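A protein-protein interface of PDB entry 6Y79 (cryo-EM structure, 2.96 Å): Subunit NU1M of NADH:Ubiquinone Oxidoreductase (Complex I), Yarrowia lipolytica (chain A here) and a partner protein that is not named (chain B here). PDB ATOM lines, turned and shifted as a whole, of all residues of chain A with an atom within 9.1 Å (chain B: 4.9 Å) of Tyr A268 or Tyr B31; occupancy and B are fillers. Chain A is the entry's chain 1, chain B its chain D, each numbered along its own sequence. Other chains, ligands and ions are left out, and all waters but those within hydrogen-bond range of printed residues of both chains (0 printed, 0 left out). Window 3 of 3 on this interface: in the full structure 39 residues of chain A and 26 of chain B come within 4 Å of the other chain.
O of Val B30 sits at hydrogen-bond distance from N of Gly B35.
CG2 of Ile A3 touches NH1 of Arg B32, at 3.6 Å.
Arg B32 touches Asn A4 (NH1 to CA, 3.4 Å).
Tyr A268 touches Val B27.
Tyr B31 touches Tyr A268.
Phe A271 touches Val B30 (CD2 to CG1, 3.5 Å).
CZ of Phe A271 touches O of Gly B35, 3.4 Å away.
N of Leu A272 touches CG2 of Val B27, 3.6 Å away.
Tyr A268 touches just these residues of chain B: Val B27 (3.8 Å) and Tyr B31 (3.9 Å).
Tyr B31 touches one residue of chain A.
Val B30 touches just one residue of chain A: Phe A271.
Printed residues of chain A within 4 Å of Gly B35: Phe A271.
Printed residues of chain B within 4 Å of Phe A271: Val B30 (3.5 Å) and Gly B35 (3.4 Å).
Of the printed residues of chain B, Leu A272 touches Val B27.
Of the printed residues of chain A, Arg B32 touches Ile A3 and Asn A4.
Printed residues of chain B within 4 Å of Asn A4: Arg B32.
Gly B34 touches none of the printed residues of chain A.
Val A269 touches none of the printed residues of chain B.
The nearest residue of chain A that does not touch Tyr B31 is Ile A3 (4.1 Å).
The nearest printed residue of chain B that does not touch Ile A3 is Tyr B31 (4.1 Å).
Of the 17 printed residues of chain A, 5 touch a printed residue of chain B.
Hydrophobic or aromatic side chains of chain A that line the printed part of chain B: Ile A3, Tyr A268, Phe A271 and Leu A272.
Printed residues of chain B that touch a printed residue of chain A: Val B27, Val B30, Tyr B31, Arg B32 and Gly B35.
Hydrophobic or aromatic side chains of chain B within 4 Å of the printed part of chain A: Val B27, Val B30 and Tyr B31.
Among the printed residues, 7 pairs touch across the chains.
Among the printed residues, no Asp or Glu carboxylate lies within 4 Å of a Lys or Arg side-chain nitrogen of the other chain.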
ATOM      1  N   ILE A   2      -1.427   7.865   4.826  1.00  0.00           N
ATOM      2  CA  ILE A   2      -2.790   8.262   4.512  1.00  0.00           C
ATOM      3  C   ILE A   2      -2.758   9.327   3.425  1.00  0.00           C
ATOM      4  O   ILE A   2      -3.596   9.313   2.505  1.00  0.00           O
ATOM      5  CB  ILE A   2      -3.502   8.740   5.792  1.00  0.00           C
ATOM      6  CG1 ILE A   2      -3.447   7.640   6.859  1.00  0.00           C
ATOM      7  CG2 ILE A   2      -4.942   9.121   5.516  1.00  0.00           C
ATOM      8  CD1 ILE A   2      -4.126   6.353   6.456  1.00  0.00           C
ATOM      9  N   ILE A   3      -1.721  10.169   3.458  1.00  0.00           N
ATOM     10  CA  ILE A   3      -1.615  11.350   2.612  1.00  0.00           C
ATOM     11  C   ILE A   3      -1.458  10.971   1.140  1.00  0.00           C
ATOM     12  O   ILE A   3      -2.175  11.476   0.273  1.00  0.00           O
ATOM     13  CB  ILE A   3      -0.427  12.191   3.118  1.00  0.00           C
ATOM     14  CG1 ILE A   3      -0.409  12.269   4.668  1.00  0.00           C
ATOM     15  CG2 ILE A   3      -0.437  13.561   2.491  1.00  0.00           C
ATOM     16  CD1 ILE A   3      -1.588  12.977   5.320  1.00  0.00           C
ATOM     17  N   ASN A   4      -0.546  10.060   0.825  1.00  0.00           N
ATOM     18  CA  ASN A   4      -0.289   9.775  -0.581  1.00  0.00           C
ATOM     19  C   ASN A   4      -1.364   8.900  -1.214  1.00  0.00           C
ATOM     20  O   ASN A   4      -1.641   9.054  -2.406  1.00  0.00           O
ATOM     21  CB  ASN A   4       1.101   9.160  -0.740  1.00  0.00           C
ATOM     22  CG  ASN A   4       1.243   7.858  -0.005  1.00  0.00           C
ATOM     23  OD1 ASN A   4       0.434   7.531   0.859  1.00  0.00           O
ATOM     24  ND2 ASN A   4       2.288   7.115  -0.317  1.00  0.00           N
ATOM     25  N   VAL A   6      -4.586   8.979  -0.318  1.00  0.00           N
ATOM     26  CA  VAL A   6      -5.726   9.861  -0.577  1.00  0.00           C
ATOM     27  C   VAL A   6      -5.423  10.752  -1.779  1.00  0.00           C
ATOM     28  O   VAL A   6      -6.290  10.923  -2.639  1.00  0.00           O
ATOM     29  CB  VAL A   6      -6.183  10.663   0.677  1.00  0.00           C
ATOM     30  CG1 VAL A   6      -5.237  11.752   1.118  1.00  0.00           C
ATOM     31  CG2 VAL A   6      -7.534  11.295   0.422  1.00  0.00           C
ATOM     32  N   PHE A 263      -4.482  38.763  -0.668  1.00  0.00           N
ATOM     33  CA  PHE A 263      -4.014  38.066   0.520  1.00  0.00           C
ATOM     34  C   PHE A 263      -3.046  38.917   1.327  1.00  0.00           C
ATOM     35  O   PHE A 263      -2.625  39.997   0.914  1.00  0.00           O
ATOM     36  CB  PHE A 263      -3.350  36.750   0.137  1.00  0.00           C
ATOM     37  CG  PHE A 263      -4.284  35.775  -0.490  1.00  0.00           C
ATOM     38  CD1 PHE A 263      -5.160  35.045   0.286  1.00  0.00           C
ATOM     39  CD2 PHE A 263      -4.295  35.596  -1.859  1.00  0.00           C
ATOM     40  CE1 PHE A 263      -6.026  34.149  -0.293  1.00  0.00           C
ATOM     41  CE2 PHE A 263      -5.159  34.702  -2.443  1.00  0.00           C
ATOM     42  CZ  PHE A 263      -6.024  33.978  -1.660  1.00  0.00           C
ATOM     43  N   ASP A 265      -0.908  36.853   3.954  1.00  0.00           N
ATOM     44  CA  ASP A 265       0.121  35.866   4.263  1.00  0.00           C
ATOM     45  C   ASP A 265      -0.338  34.497   3.778  1.00  0.00           C
ATOM     46  O   ASP A 265      -1.520  34.278   3.503  1.00  0.00           O
ATOM     47  CB  ASP A 265       0.455  35.827   5.764  1.00  0.00           C
ATOM     48  CG  ASP A 265       1.811  35.188   6.042  1.00  0.00           C
ATOM     49  OD1 ASP A 265       2.572  35.017   5.067  1.00  0.00           O
ATOM     50  OD2 ASP A 265       2.107  34.838   7.204  1.00  0.00           O
ATOM     51  N   TYR A 266       0.631  33.583   3.683  1.00  0.00           N
ATOM     52  CA  TYR A 266       0.414  32.202   3.267  1.00  0.00           C
ATOM     53  C   TYR A 266      -0.561  31.492   4.196  1.00  0.00           C
ATOM     54  O   TYR A 266      -0.294  31.339   5.392  1.00  0.00           O
ATOM     55  CB  TYR A 266       1.748  31.461   3.251  1.00  0.00           C
ATOM     56  CG  TYR A 266       2.717  32.018   2.254  1.00  0.00           C
ATOM     57  CD1 TYR A 266       2.605  31.701   0.912  1.00  0.00           C
ATOM     58  CD2 TYR A 266       3.733  32.872   2.647  1.00  0.00           C
ATOM     59  CE1 TYR A 266       3.483  32.215  -0.015  1.00  0.00           C
ATOM     60  CE2 TYR A 266       4.617  33.388   1.725  1.00  0.00           C
ATOM     61  CZ  TYR A 266       4.484  33.057   0.397  1.00  0.00           C
ATOM     62  OH  TYR A 266       5.361  33.569  -0.524  1.00  0.00           O
ATOM     63  N   SER A 267      -1.678  31.048   3.634  1.00  0.00           N
ATOM     64  CA  SER A 267      -2.659  30.247   4.341  1.00  0.00           C
ATOM     65  C   SER A 267      -3.069  29.129   3.402  1.00  0.00           C
ATOM     66  O   SER A 267      -2.736  29.148   2.218  1.00  0.00           O
ATOM     67  CB  SER A 267      -3.864  31.087   4.766  1.00  0.00           C
ATOM     68  OG  SER A 267      -3.453  32.189   5.554  1.00  0.00           O
ATOM     69  N   TYR A 268      -3.809  28.153   3.935  1.00  0.00           N
ATOM     70  CA  TYR A 268      -4.253  27.037   3.107  1.00  0.00           C
ATOM     71  C   TYR A 268      -5.254  27.479   2.049  1.00  0.00           C
ATOM     72  O   TYR A 268      -5.347  26.850   0.989  1.00  0.00           O
ATOM     73  CB  TYR A 268      -4.857  25.940   3.976  1.00  0.00           C
ATOM     74  CG  TYR A 268      -3.854  25.221   4.839  1.00  0.00           C
ATOM     75  CD1 TYR A 268      -3.067  24.200   4.321  1.00  0.00           C
ATOM     76  CD2 TYR A 268      -3.696  25.560   6.175  1.00  0.00           C
ATOM     77  CE1 TYR A 268      -2.148  23.536   5.110  1.00  0.00           C
ATOM     78  CE2 TYR A 268      -2.781  24.900   6.976  1.00  0.00           C
ATOM     79  CZ  TYR A 268      -2.009  23.890   6.436  1.00  0.00           C
ATOM     80  OH  TYR A 268      -1.097  23.235   7.230  1.00  0.00           O
ATOM     81  N   VAL A 269      -5.981  28.570   2.297  1.00  0.00           N
ATOM     82  CA  VAL A 269      -6.884  29.090   1.280  1.00  0.00           C
ATOM     83  C   VAL A 269      -6.097  29.773   0.164  1.00  0.00           C
ATOM     84  O   VAL A 269      -6.518  29.752  -0.997  1.00  0.00           O
ATOM     85  CB  VAL A 269      -7.936  30.016   1.930  1.00  0.00           C
ATOM     86  CG1 VAL A 269      -7.305  31.269   2.513  1.00  0.00           C
ATOM     87  CG2 VAL A 269      -9.050  30.365   0.953  1.00  0.00           C
ATOM     88  N   SER A 270      -4.909  30.310   0.464  1.00  0.00           N
ATOM     89  CA  SER A 270      -4.104  30.937  -0.580  1.00  0.00           C
ATOM     90  C   SER A 270      -3.451  29.895  -1.476  1.00  0.00           C
ATOM     91  O   SER A 270      -3.395  30.068  -2.699  1.00  0.00           O
ATOM     92  CB  SER A 270      -3.049  31.844   0.041  1.00  0.00           C
ATOM     93  OG  SER A 270      -2.266  32.456  -0.964  1.00  0.00           O
ATOM     94  N   PHE A 271      -2.968  28.797  -0.888  1.00  0.00           N
ATOM     95  CA  PHE A 271      -2.469  27.686  -1.688  1.00  0.00           C
ATOM     96  C   PHE A 271      -3.588  27.013  -2.466  1.00  0.00           C
ATOM     97  O   PHE A 271      -3.368  26.561  -3.597  1.00  0.00           O
ATOM     98  CB  PHE A 271      -1.759  26.672  -0.796  1.00  0.00           C
ATOM     99  CG  PHE A 271      -0.481  27.181  -0.198  1.00  0.00           C
ATOM    100  CD1 PHE A 271       0.615  27.450  -0.999  1.00  0.00           C
ATOM    101  CD2 PHE A 271      -0.375  27.387   1.164  1.00  0.00           C
ATOM    102  CE1 PHE A 271       1.788  27.918  -0.451  1.00  0.00           C
ATOM    103  CE2 PHE A 271       0.794  27.853   1.719  1.00  0.00           C
ATOM    104  CZ  PHE A 271       1.877  28.118   0.911  1.00  0.00           C
ATOM    105  N   LEU A 272      -4.794  26.967  -1.891  1.00  0.00           N
ATOM    106  CA  LEU A 272      -5.958  26.439  -2.597  1.00  0.00           C
ATOM    107  C   LEU A 272      -6.292  27.287  -3.811  1.00  0.00           C
ATOM    108  O   LEU A 272      -6.517  26.766  -4.907  1.00  0.00           O
ATOM    109  CB  LEU A 272      -7.141  26.370  -1.632  1.00  0.00           C
ATOM    110  CG  LEU A 272      -8.517  25.929  -2.117  1.00  0.00           C
ATOM    111  CD1 LEU A 272      -8.467  24.502  -2.608  1.00  0.00           C
ATOM    112  CD2 LEU A 272      -9.513  26.069  -0.979  1.00  0.00           C
ATOM    113  N   PHE A 273      -6.279  28.607  -3.633  1.00  0.00           N
ATOM    114  CA  PHE A 273      -6.560  29.540  -4.715  1.00  0.00           C
ATOM    115  C   PHE A 273      -5.499  29.468  -5.807  1.00  0.00           C
ATOM    116  O   PHE A 273      -5.828  29.477  -7.000  1.00  0.00           O
ATOM    117  CB  PHE A 273      -6.654  30.943  -4.121  1.00  0.00           C
ATOM    118  CG  PHE A 273      -7.178  31.971  -5.059  1.00  0.00           C
ATOM    119  CD1 PHE A 273      -8.434  31.841  -5.619  1.00  0.00           C
ATOM    120  CD2 PHE A 273      -6.434  33.095  -5.348  1.00  0.00           C
ATOM    121  CE1 PHE A 273      -8.923  32.805  -6.480  1.00  0.00           C
ATOM    122  CE2 PHE A 273      -6.921  34.062  -6.203  1.00  0.00           C
ATOM    123  CZ  PHE A 273      -8.162  33.916  -6.769  1.00  0.00           C
ATOM    124  N   GLU A 274      -4.229  29.345  -5.415  1.00  0.00           N
ATOM    125  CA  GLU A 274      -3.142  29.262  -6.388  1.00  0.00           C
ATOM    126  C   GLU A 274      -3.192  27.964  -7.188  1.00  0.00           C
ATOM    127  O   GLU A 274      -2.982  27.975  -8.408  1.00  0.00           O
ATOM    128  CB  GLU A 274      -1.805  29.394  -5.672  1.00  0.00           C
ATOM    129  CG  GLU A 274      -0.615  29.395  -6.592  1.00  0.00           C
ATOM    130  CD  GLU A 274       0.686  29.549  -5.841  1.00  0.00           C
ATOM    131  OE1 GLU A 274       0.641  29.690  -4.604  1.00  0.00           O
ATOM    132  OE2 GLU A 274       1.755  29.532  -6.485  1.00  0.00           O
ATOM    133  N   GLY A 275      -3.472  26.839  -6.522  1.00  0.00           N
ATOM    134  CA  GLY A 275      -3.647  25.588  -7.235  1.00  0.00           C
ATOM    135  C   GLY A 275      -4.848  25.592  -8.157  1.00  0.00           C
ATOM    136  O   GLY A 275      -4.796  25.005  -9.244  1.00  0.00           O
ATOM    137  N   LEU A 276      -5.928  26.273  -7.748  1.00  0.00           N
ATOM    138  CA  LEU A 276      -7.086  26.446  -8.618  1.00  0.00           C
ATOM    139  C   LEU A 276      -6.722  27.209  -9.884  1.00  0.00           C
ATOM    140  O   LEU A 276      -7.099  26.795 -10.985  1.00  0.00           O
ATOM    141  CB  LEU A 276      -8.203  27.176  -7.875  1.00  0.00           C
ATOM    142  CG  LEU A 276      -9.098  26.424  -6.894  1.00  0.00           C
ATOM    143  CD1 LEU A 276     -10.192  27.352  -6.401  1.00  0.00           C
ATOM    144  CD2 LEU A 276      -9.679  25.175  -7.514  1.00  0.00           C
ATOM    145  N   VAL B  27      -3.031  21.583  -2.165  1.00  0.00           N
ATOM    146  CA  VAL B  27      -3.185  21.730  -0.716  1.00  0.00           C
ATOM    147  C   VAL B  27      -2.712  20.473   0.013  1.00  0.00           C
ATOM    148  O   VAL B  27      -2.130  20.558   1.102  1.00  0.00           O
ATOM    149  CB  VAL B  27      -4.635  22.119  -0.373  1.00  0.00           C
ATOM    150  CG1 VAL B  27      -4.958  21.964   1.107  1.00  0.00           C
ATOM    151  CG2 VAL B  27      -4.822  23.544  -0.722  1.00  0.00           C
ATOM    152  N   LEU B  28      -2.869  19.299  -0.610  1.00  0.00           N
ATOM    153  CA  LEU B  28      -2.317  18.074  -0.028  1.00  0.00           C
ATOM    154  C   LEU B  28      -0.791  18.105   0.020  1.00  0.00           C
ATOM    155  O   LEU B  28      -0.187  17.672   1.010  1.00  0.00           O
ATOM    156  CB  LEU B  28      -2.806  16.860  -0.813  1.00  0.00           C
ATOM    157  CG  LEU B  28      -4.245  16.430  -0.535  1.00  0.00           C
ATOM    158  CD1 LEU B  28      -4.642  15.269  -1.416  1.00  0.00           C
ATOM    159  CD2 LEU B  28      -4.428  16.081   0.927  1.00  0.00           C
ATOM    160  N   HIS B  29      -0.156  18.656  -1.017  1.00  0.00           N
ATOM    161  CA  HIS B  29       1.300  18.792  -1.023  1.00  0.00           C
ATOM    162  C   HIS B  29       1.781  19.772   0.039  1.00  0.00           C
ATOM    163  O   HIS B  29       2.791  19.525   0.709  1.00  0.00           O
ATOM    164  CB  HIS B  29       1.775  19.252  -2.395  1.00  0.00           C
ATOM    165  CG  HIS B  29       1.872  18.153  -3.401  1.00  0.00           C
ATOM    166  ND1 HIS B  29       2.756  17.105  -3.279  1.00  0.00           N
ATOM    167  CD2 HIS B  29       1.201  17.945  -4.555  1.00  0.00           C
ATOM    168  CE1 HIS B  29       2.617  16.294  -4.310  1.00  0.00           C
ATOM    169  NE2 HIS B  29       1.678  16.779  -5.099  1.00  0.00           N
ATOM    170  N   VAL B  30       1.077  20.893   0.195  1.00  0.00           N
ATOM    171  CA  VAL B  30       1.476  21.893   1.181  1.00  0.00           C
ATOM    172  C   VAL B  30       1.258  21.370   2.596  1.00  0.00           C
ATOM    173  O   VAL B  30       2.065  21.627   3.500  1.00  0.00           O
ATOM    174  CB  VAL B  30       0.722  23.206   0.915  1.00  0.00           C
ATOM    175  CG1 VAL B  30       0.993  24.219   1.983  1.00  0.00           C
ATOM    176  CG2 VAL B  30       1.165  23.771  -0.386  1.00  0.00           C
ATOM    177  N   TYR B  31       0.196  20.586   2.800  1.00  0.00           N
ATOM    178  CA  TYR B  31      -0.023  19.950   4.093  1.00  0.00           C
ATOM    179  C   TYR B  31       1.039  18.905   4.388  1.00  0.00           C
ATOM    180  O   TYR B  31       1.409  18.715   5.551  1.00  0.00           O
ATOM    181  CB  TYR B  31      -1.409  19.312   4.147  1.00  0.00           C
ATOM    182  CG  TYR B  31      -1.710  18.689   5.489  1.00  0.00           C
ATOM    183  CD1 TYR B  31      -1.969  19.485   6.598  1.00  0.00           C
ATOM    184  CD2 TYR B  31      -1.711  17.310   5.655  1.00  0.00           C
ATOM    185  CE1 TYR B  31      -2.229  18.927   7.829  1.00  0.00           C
ATOM    186  CE2 TYR B  31      -1.969  16.744   6.882  1.00  0.00           C
ATOM    187  CZ  TYR B  31      -2.230  17.555   7.965  1.00  0.00           C
ATOM    188  OH  TYR B  31      -2.492  16.994   9.192  1.00  0.00           O
ATOM    189  N   ARG B  32       1.539  18.223   3.356  1.00  0.00           N
ATOM    190  CA  ARG B  32       2.647  17.296   3.561  1.00  0.00           C
ATOM    191  C   ARG B  32       3.929  18.030   3.943  1.00  0.00           C
ATOM    192  O   ARG B  32       4.645  17.600   4.853  1.00  0.00           O
ATOM    193  CB  ARG B  32       2.864  16.456   2.308  1.00  0.00           C
ATOM    194  CG  ARG B  32       4.054  15.528   2.395  1.00  0.00           C
ATOM    195  CD  ARG B  32       4.172  14.700   1.146  1.00  0.00           C
ATOM    196  NE  ARG B  32       2.953  13.945   0.902  1.00  0.00           N
ATOM    197  CZ  ARG B  32       2.703  13.286  -0.221  1.00  0.00           C
ATOM    198  NH1 ARG B  32       1.570  12.623  -0.366  1.00  0.00           N
ATOM    199  NH2 ARG B  32       3.589  13.292  -1.200  1.00  0.00           N
ATOM    200  N   ASN B  33       4.232  19.146   3.272  1.00  0.00           N
ATOM    201  CA  ASN B  33       5.465  19.867   3.583  1.00  0.00           C
ATOM    202  C   ASN B  33       5.395  20.589   4.921  1.00  0.00           C
ATOM    203  O   ASN B  33       6.419  20.742   5.593  1.00  0.00           O
ATOM    204  CB  ASN B  33       5.786  20.875   2.490  1.00  0.00           C
ATOM    205  CG  ASN B  33       6.105  20.221   1.185  1.00  0.00           C
ATOM    206  OD1 ASN B  33       5.495  20.525   0.169  1.00  0.00           O
ATOM    207  ND2 ASN B  33       7.063  19.308   1.199  1.00  0.00           N
ATOM    208  N   GLY B  34       4.218  21.049   5.318  1.00  0.00           N
ATOM    209  CA  GLY B  34       4.103  21.790   6.554  1.00  0.00           C
ATOM    210  C   GLY B  34       3.957  23.278   6.334  1.00  0.00           C
ATOM    211  O   GLY B  34       4.451  24.084   7.128  1.00  0.00           O
ATOM    212  N   GLY B  35       3.291  23.658   5.246  1.00  0.00           N
ATOM    213  CA  GLY B  35       2.944  25.041   5.002  1.00  0.00           C
ATOM    214  C   GLY B  35       3.706  25.720   3.891  1.00  0.00           C
ATOM    215  O   GLY B  35       3.494  26.917   3.669  1.00  0.00           O
